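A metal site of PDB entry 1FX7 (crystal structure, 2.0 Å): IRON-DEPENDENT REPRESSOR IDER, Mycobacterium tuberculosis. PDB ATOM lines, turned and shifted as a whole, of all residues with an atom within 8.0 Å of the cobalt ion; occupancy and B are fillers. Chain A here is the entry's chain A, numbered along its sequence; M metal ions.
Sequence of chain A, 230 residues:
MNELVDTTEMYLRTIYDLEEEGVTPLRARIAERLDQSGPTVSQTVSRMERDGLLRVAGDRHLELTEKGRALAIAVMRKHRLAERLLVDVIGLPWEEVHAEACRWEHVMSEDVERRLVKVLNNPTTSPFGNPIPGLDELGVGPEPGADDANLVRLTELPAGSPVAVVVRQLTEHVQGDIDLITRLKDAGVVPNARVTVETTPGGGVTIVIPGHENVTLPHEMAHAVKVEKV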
ATOM      1  N   ARG A  13     -22.546  28.258  13.557  1.00  0.00           N
ATOM      2  CA  ARG A  13     -22.024  27.059  14.197  1.00  0.00           C
ATOM      3  C   ARG A  13     -21.942  25.867  13.262  1.00  0.00           C
ATOM      4  O   ARG A  13     -21.063  25.038  13.534  1.00  0.00           O
ATOM      5  CB  ARG A  13     -22.785  26.680  15.479  1.00  0.00           C
ATOM      6  CG  ARG A  13     -21.841  25.962  16.455  1.00  0.00           C
ATOM      7  CD  ARG A  13     -22.608  25.035  17.368  1.00  0.00           C
ATOM      8  NE  ARG A  13     -22.917  23.777  16.698  1.00  0.00           N
ATOM      9  CZ  ARG A  13     -24.004  23.051  16.873  1.00  0.00           C
ATOM     10  NH1 ARG A  13     -24.956  23.427  17.723  1.00  0.00           N
ATOM     11  NH2 ARG A  13     -24.193  21.916  16.193  1.00  0.00           N
ATOM     12  N   ASP A  17     -18.610  23.688  12.934  1.00  0.00           N
ATOM     13  CA  ASP A  17     -18.705  22.246  13.057  1.00  0.00           C
ATOM     14  C   ASP A  17     -18.010  21.535  11.883  1.00  0.00           C
ATOM     15  O   ASP A  17     -17.192  20.658  12.051  1.00  0.00           O
ATOM     16  CB  ASP A  17     -20.164  21.789  12.989  1.00  0.00           C
ATOM     17  CG  ASP A  17     -20.990  21.980  14.241  1.00  0.00           C
ATOM     18  OD1 ASP A  17     -20.481  22.166  15.356  1.00  0.00           O
ATOM     19  OD2 ASP A  17     -22.231  21.937  14.124  1.00  0.00           O
ATOM     20  N   MET A  76     -20.708  28.226  20.247  1.00  0.00           N
ATOM     21  CA  MET A  76     -20.138  26.936  20.635  1.00  0.00           C
ATOM     22  C   MET A  76     -19.762  26.896  22.105  1.00  0.00           C
ATOM     23  O   MET A  76     -19.973  25.886  22.764  1.00  0.00           O
ATOM     24  CB  MET A  76     -18.906  26.626  19.788  1.00  0.00           C
ATOM     25  CG  MET A  76     -18.401  25.195  19.895  1.00  0.00           C
ATOM     26  SD  MET A  76     -19.667  24.011  19.373  1.00  0.00           S
ATOM     27  CE  MET A  76     -20.249  23.398  20.946  1.00  0.00           C
ATOM     28  N   HIS A  79     -22.852  26.429  23.875  1.00  0.00           N
ATOM     29  CA  HIS A  79     -23.332  25.060  23.687  1.00  0.00           C
ATOM     30  C   HIS A  79     -22.654  24.099  24.652  1.00  0.00           C
ATOM     31  O   HIS A  79     -23.286  23.284  25.323  1.00  0.00           O
ATOM     32  CB  HIS A  79     -22.967  24.633  22.262  1.00  0.00           C
ATOM     33  CG  HIS A  79     -23.430  23.239  21.953  1.00  0.00           C
ATOM     34  ND1 HIS A  79     -24.709  22.973  21.528  1.00  0.00           N
ATOM     35  CD2 HIS A  79     -22.791  22.041  21.995  1.00  0.00           C
ATOM     36  CE1 HIS A  79     -24.852  21.681  21.336  1.00  0.00           C
ATOM     37  NE2 HIS A  79     -23.698  21.097  21.608  1.00  0.00           N
ATOM     38  N   ARG A  80     -21.315  24.168  24.679  1.00  0.00           N
ATOM     39  CA  ARG A  80     -20.535  23.197  25.450  1.00  0.00           C
ATOM     40  C   ARG A  80     -20.599  23.428  26.956  1.00  0.00           C
ATOM     41  O   ARG A  80     -20.606  22.434  27.669  1.00  0.00           O
ATOM     42  CB  ARG A  80     -19.124  23.049  24.872  1.00  0.00           C
ATOM     43  CG  ARG A  80     -19.102  22.487  23.455  1.00  0.00           C
ATOM     44  CD  ARG A  80     -17.731  22.361  22.810  1.00  0.00           C
ATOM     45  NE  ARG A  80     -17.850  21.721  21.495  1.00  0.00           N
ATOM     46  CZ  ARG A  80     -17.028  21.759  20.462  1.00  0.00           C
ATOM     47  NH1 ARG A  80     -15.893  22.430  20.458  1.00  0.00           N
ATOM     48  NH2 ARG A  80     -17.374  21.121  19.347  1.00  0.00           N
ATOM     49  N   GLU A  83     -23.972  21.874  27.818  1.00  0.00           N
ATOM     50  CA  GLU A  83     -23.796  20.425  27.924  1.00  0.00           C
ATOM     51  C   GLU A  83     -23.186  20.019  29.264  1.00  0.00           C
ATOM     52  O   GLU A  83     -23.677  19.050  29.853  1.00  0.00           O
ATOM     53  CB  GLU A  83     -22.953  19.864  26.778  1.00  0.00           C
ATOM     54  CG  GLU A  83     -23.715  19.867  25.452  1.00  0.00           C
ATOM     55  CD  GLU A  83     -22.940  19.358  24.266  1.00  0.00           C
ATOM     56  OE1 GLU A  83     -21.698  19.502  24.251  1.00  0.00           O
ATOM     57  OE2 GLU A  83     -23.537  18.795  23.316  1.00  0.00           O
ATOM     58  N   TRP A  94     -26.655  11.494  29.057  1.00  0.00           N
ATOM     59  CA  TRP A  94     -25.584  12.017  28.187  1.00  0.00           C
ATOM     60  C   TRP A  94     -26.007  12.098  26.731  1.00  0.00           C
ATOM     61  O   TRP A  94     -25.757  13.116  26.086  1.00  0.00           O
ATOM     62  CB  TRP A  94     -24.355  11.173  28.351  1.00  0.00           C
ATOM     63  CG  TRP A  94     -23.062  11.385  27.646  1.00  0.00           C
ATOM     64  CD1 TRP A  94     -22.008  12.156  28.055  1.00  0.00           C
ATOM     65  CD2 TRP A  94     -22.646  10.766  26.420  1.00  0.00           C
ATOM     66  NE1 TRP A  94     -20.967  12.062  27.166  1.00  0.00           N
ATOM     67  CE2 TRP A  94     -21.328  11.212  26.145  1.00  0.00           C
ATOM     68  CE3 TRP A  94     -23.261   9.890  25.527  1.00  0.00           C
ATOM     69  CZ2 TRP A  94     -20.620  10.805  25.030  1.00  0.00           C
ATOM     70  CZ3 TRP A  94     -22.547   9.477  24.407  1.00  0.00           C
ATOM     71  CH2 TRP A  94     -21.242   9.935  24.160  1.00  0.00           C
ATOM     72  N   VAL A  97     -28.289  15.372  25.999  1.00  0.00           N
ATOM     73  CA  VAL A  97     -27.855  16.740  26.270  1.00  0.00           C
ATOM     74  C   VAL A  97     -27.583  17.546  24.998  1.00  0.00           C
ATOM     75  O   VAL A  97     -27.794  18.751  25.001  1.00  0.00           O
ATOM     76  CB  VAL A  97     -26.637  16.785  27.214  1.00  0.00           C
ATOM     77  CG1 VAL A  97     -26.908  15.957  28.474  1.00  0.00           C
ATOM     78  CG2 VAL A  97     -25.369  16.338  26.525  1.00  0.00           C
ATOM     79  N   HIS A  98     -27.070  16.923  23.938  1.00  0.00           N
ATOM     80  CA  HIS A  98     -26.771  17.692  22.720  1.00  0.00           C
ATOM     81  C   HIS A  98     -28.001  18.378  22.158  1.00  0.00           C
ATOM     82  O   HIS A  98     -27.904  19.590  21.834  1.00  0.00           O
ATOM     83  CB  HIS A  98     -26.073  16.808  21.670  1.00  0.00           C
ATOM     84  CG  HIS A  98     -25.932  17.584  20.386  1.00  0.00           C
ATOM     85  ND1 HIS A  98     -24.984  18.558  20.227  1.00  0.00           N
ATOM     86  CD2 HIS A  98     -26.662  17.528  19.236  1.00  0.00           C
ATOM     87  CE1 HIS A  98     -25.122  19.073  19.012  1.00  0.00           C
ATOM     88  NE2 HIS A  98     -26.132  18.462  18.395  1.00  0.00           N
ATOM     89  N   ALA A  99     -29.129  17.687  21.988  1.00  0.00           N
ATOM     90  CA  ALA A  99     -30.289  18.371  21.393  1.00  0.00           C
ATOM     91  C   ALA A  99     -30.778  19.509  22.285  1.00  0.00           C
ATOM     92  O   ALA A  99     -31.186  20.578  21.804  1.00  0.00           O
ATOM     93  CB  ALA A  99     -31.397  17.382  21.063  1.00  0.00           C
ATOM     94  N   GLU A 100     -30.764  19.302  23.593  1.00  0.00           N
ATOM     95  CA  GLU A 100     -31.162  20.349  24.538  1.00  0.00           C
ATOM     96  C   GLU A 100     -30.235  21.550  24.415  1.00  0.00           C
ATOM     97  O   GLU A 100     -30.639  22.698  24.220  1.00  0.00           O
ATOM     98  CB  GLU A 100     -31.107  19.776  25.953  1.00  0.00           C
ATOM     99  CG  GLU A 100     -31.701  20.700  27.012  1.00  0.00           C
ATOM    100  CD  GLU A 100     -33.205  20.529  27.165  1.00  0.00           C
ATOM    101  OE1 GLU A 100     -33.691  19.389  27.044  1.00  0.00           O
ATOM    102  OE2 GLU A 100     -33.921  21.518  27.426  1.00  0.00           O
ATOM    103  N   ALA A 101     -28.925  21.289  24.469  1.00  0.00           N
ATOM    104  CA  ALA A 101     -27.930  22.366  24.356  1.00  0.00           C
ATOM    105  C   ALA A 101     -27.981  23.070  23.001  1.00  0.00           C
ATOM    106  O   ALA A 101     -27.671  24.264  22.928  1.00  0.00           O
ATOM    107  CB  ALA A 101     -26.514  21.830  24.594  1.00  0.00           C
ATOM    108  N   CYS A 102     -28.409  22.402  21.926  1.00  0.00           N
ATOM    109  CA  CYS A 102     -28.514  23.052  20.629  1.00  0.00           C
ATOM    110  C   CYS A 102     -29.585  24.155  20.657  1.00  0.00           C
ATOM    111  O   CYS A 102     -29.530  25.094  19.855  1.00  0.00           O
ATOM    112  CB  CYS A 102     -28.817  22.120  19.450  1.00  0.00           C
ATOM    113  SG  CYS A 102     -28.515  22.911  17.838  1.00  0.00           S
ATOM    114  N   GLU A 105     -27.992  27.023  23.573  1.00  0.00           N
ATOM    115  CA  GLU A 105     -26.865  27.843  23.131  1.00  0.00           C
ATOM    116  C   GLU A 105     -27.299  29.180  22.577  1.00  0.00           C
ATOM    117  O   GLU A 105     -26.468  30.075  22.475  1.00  0.00           O
ATOM    118  CB  GLU A 105     -26.064  27.051  22.052  1.00  0.00           C
ATOM    119  CG  GLU A 105     -26.830  26.939  20.724  1.00  0.00           C
ATOM    120  CD  GLU A 105     -26.211  25.904  19.799  1.00  0.00           C
ATOM    121  OE1 GLU A 105     -25.132  25.392  20.112  1.00  0.00           O
ATOM    122  OE2 GLU A 105     -26.794  25.545  18.744  1.00  0.00           O
ATOM    123  N   SER A 126     -16.215  19.740  26.707  1.00  0.00           N
ATOM    124  CA  SER A 126     -17.628  19.319  26.870  1.00  0.00           C
ATOM    125  C   SER A 126     -17.616  17.868  27.304  1.00  0.00           C
ATOM    126  O   SER A 126     -16.568  17.193  27.287  1.00  0.00           O
ATOM    127  CB  SER A 126     -18.356  19.545  25.534  1.00  0.00           C
ATOM    128  OG  SER A 126     -18.032  18.434  24.657  1.00  0.00           O
ATOM    129  N   PRO A 127     -18.767  17.295  27.644  1.00  0.00           N
ATOM    130  CA  PRO A 127     -18.902  15.896  27.990  1.00  0.00           C
ATOM    131  C   PRO A 127     -18.614  14.936  26.845  1.00  0.00           C
ATOM    132  O   PRO A 127     -18.556  13.710  27.055  1.00  0.00           O
ATOM    133  CB  PRO A 127     -20.356  15.712  28.397  1.00  0.00           C
ATOM    134  CG  PRO A 127     -20.942  17.071  28.490  1.00  0.00           C
ATOM    135  CD  PRO A 127     -20.076  17.980  27.667  1.00  0.00           C
ATOM    136  N   PHE A 128     -18.465  15.433  25.627  1.00  0.00           N
ATOM    137  CA  PHE A 128     -18.124  14.677  24.438  1.00  0.00           C
ATOM    138  C   PHE A 128     -16.640  14.816  24.114  1.00  0.00           C
ATOM    139  O   PHE A 128     -16.137  14.378  23.073  1.00  0.00           O
ATOM    140  CB  PHE A 128     -18.985  15.152  23.234  1.00  0.00           C
ATOM    141  CG  PHE A 128     -20.430  14.897  23.599  1.00  0.00           C
ATOM    142  CD1 PHE A 128     -21.169  15.903  24.206  1.00  0.00           C
ATOM    143  CD2 PHE A 128     -20.991  13.657  23.400  1.00  0.00           C
ATOM    144  CE1 PHE A 128     -22.478  15.675  24.579  1.00  0.00           C
ATOM    145  CE2 PHE A 128     -22.308  13.427  23.766  1.00  0.00           C
ATOM    146  CZ  PHE A 128     -23.046  14.433  24.373  1.00  0.00           C
ATOM    147  N   ASN A 130     -14.818  17.593  23.594  1.00  0.00           N
ATOM    148  CA  ASN A 130     -14.403  18.713  22.769  1.00  0.00           C
ATOM    149  C   ASN A 130     -14.030  19.918  23.623  1.00  0.00           C
ATOM    150  O   ASN A 130     -14.752  20.243  24.556  1.00  0.00           O
ATOM    151  CB  ASN A 130     -15.566  19.124  21.850  1.00  0.00           C
ATOM    152  CG  ASN A 130     -16.118  17.943  21.073  1.00  0.00           C
ATOM    153  OD1 ASN A 130     -15.358  17.359  20.290  1.00  0.00           O
ATOM    154  ND2 ASN A 130     -17.393  17.592  21.232  1.00  0.00           N
ATOM    155  N   LEU A 170     -15.855  13.441  20.264  1.00  0.00           N
ATOM    156  CA  LEU A 170     -16.991  13.159  19.399  1.00  0.00           C
ATOM    157  C   LEU A 170     -17.584  14.545  19.063  1.00  0.00           C
ATOM    158  O   LEU A 170     -18.139  15.168  19.987  1.00  0.00           O
ATOM    159  CB  LEU A 170     -18.042  12.287  20.073  1.00  0.00           C
ATOM    160  CG  LEU A 170     -17.534  10.914  20.581  1.00  0.00           C
ATOM    161  CD1 LEU A 170     -17.200  10.989  22.062  1.00  0.00           C
ATOM    162  CD2 LEU A 170     -18.545   9.813  20.333  1.00  0.00           C
ATOM    163  N   THR A 171     -17.368  15.061  17.857  1.00  0.00           N
ATOM    164  CA  THR A 171     -17.814  16.417  17.528  1.00  0.00           C
ATOM    165  C   THR A 171     -19.317  16.534  17.356  1.00  0.00           C
ATOM    166  O   THR A 171     -20.014  15.541  17.508  1.00  0.00           O
ATOM    167  CB  THR A 171     -17.082  17.007  16.310  1.00  0.00           C
ATOM    168  OG1 THR A 171     -17.540  16.355  15.128  1.00  0.00           O
ATOM    169  CG2 THR A 171     -15.583  16.882  16.488  1.00  0.00           C
ATOM    170  N   GLU A 172     -19.866  17.748  17.206  1.00  0.00           N
ATOM    171  CA  GLU A 172     -21.302  17.949  17.233  1.00  0.00           C
ATOM    172  C   GLU A 172     -22.083  17.144  16.193  1.00  0.00           C
ATOM    173  O   GLU A 172     -23.206  16.741  16.480  1.00  0.00           O
ATOM    174  CB  GLU A 172     -21.669  19.456  17.134  1.00  0.00           C
ATOM    175  CG  GLU A 172     -20.844  20.320  18.080  1.00  0.00           C
ATOM    176  CD  GLU A 172     -20.990  19.911  19.538  1.00  0.00           C
ATOM    177  OE1 GLU A 172     -21.977  19.231  19.897  1.00  0.00           O
ATOM    178  OE2 GLU A 172     -20.099  20.212  20.342  1.00  0.00           O
ATOM    179  N   HIS A 173     -21.544  16.921  15.002  1.00  0.00           N
ATOM    180  CA  HIS A 173     -22.259  16.178  13.981  1.00  0.00           C
ATOM    181  C   HIS A 173     -22.643  14.776  14.415  1.00  0.00           C
ATOM    182  O   HIS A 173     -23.757  14.318  14.163  1.00  0.00           O
ATOM    183  CB  HIS A 173     -21.421  16.133  12.669  1.00  0.00           C
ATOM    184  CG  HIS A 173     -22.209  15.614  11.500  1.00  0.00           C
ATOM    185  ND1 HIS A 173     -23.486  16.068  11.227  1.00  0.00           N
ATOM    186  CD2 HIS A 173     -21.902  14.694  10.555  1.00  0.00           C
ATOM    187  CE1 HIS A 173     -23.936  15.439  10.138  1.00  0.00           C
ATOM    188  NE2 HIS A 173     -23.008  14.605   9.707  1.00  0.00           N
ATOM    189  N   VAL A 174     -21.766  14.010  15.077  1.00  0.00           N
ATOM    190  CA  VAL A 174     -22.179  12.646  15.474  1.00  0.00           C
ATOM    191  C   VAL A 174     -23.161  12.693  16.629  1.00  0.00           C
ATOM    192  O   VAL A 174     -24.109  11.913  16.716  1.00  0.00           O
ATOM    193  CB  VAL A 174     -20.989  11.730  15.715  1.00  0.00           C
ATOM    194  CG1 VAL A 174     -20.159  12.164  16.915  1.00  0.00           C
ATOM    195  CG2 VAL A 174     -21.466  10.275  15.850  1.00  0.00           C
ATOM    196  N   GLN A 175     -23.087  13.763  17.425  1.00  0.00           N
ATOM    197  CA  GLN A 175     -24.020  13.956  18.522  1.00  0.00           C
ATOM    198  C   GLN A 175     -25.422  14.229  17.985  1.00  0.00           C
ATOM    199  O   GLN A 175     -26.374  13.893  18.677  1.00  0.00           O
ATOM    200  CB  GLN A 175     -23.636  15.155  19.412  1.00  0.00           C
ATOM    201  CG  GLN A 175     -22.343  15.013  20.185  1.00  0.00           C
ATOM    202  CD  GLN A 175     -21.940  16.303  20.864  1.00  0.00           C
ATOM    203  OE1 GLN A 175     -22.759  16.992  21.446  1.00  0.00           O
ATOM    204  NE2 GLN A 175     -20.662  16.641  20.797  1.00  0.00           N
ATOM    205  N   GLY A 176     -25.541  14.826  16.808  1.00  0.00           N
ATOM    206  CA  GLY A 176     -26.819  15.201  16.214  1.00  0.00           C
ATOM    207  C   GLY A 176     -27.637  14.057  15.629  1.00  0.00           C
ATOM    208  O   GLY A 176     -28.768  14.265  15.178  1.00  0.00           O
HETATM  209 CO    CO M   1     -23.294  19.007  21.387  1.00  0.00          CO
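The side-chain amide nitrogen of Gln 175 lies within hydrogen-bond range of the backbone carbonyl oxygen of Leu 170 (3.0 Å). ND2 of Asn 130 sits close to NE2 of Gln 175 (3.4 Å). The side-chain carboxylate (OE2) of Glu 172 lies within salt-bridge range of the guanidinium group (NE) of Arg 80 (2.9 Å). The side-chain carboxylate (OE1) of Glu 105 lies within hydrogen-bond range of a ring nitrogen (ND1) of His 79 (2.8 Å).
Within 4 Å of the cobalt ion: His 79, Glu 83, His 98, Glu 172 and Gln 175. Along chain A the residues within 4 Å of the cobalt ion span positions 79 to 175.
The cobalt ion is bound by OE2 of Glu 83 (2.0 Å), OE1 of Glu 172 (2.0 Å), OE1 of Gln 175 (2.1 Å), ND1 of His 98 (2.1 Å) and NE2 of His 79 (2.1 Å).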
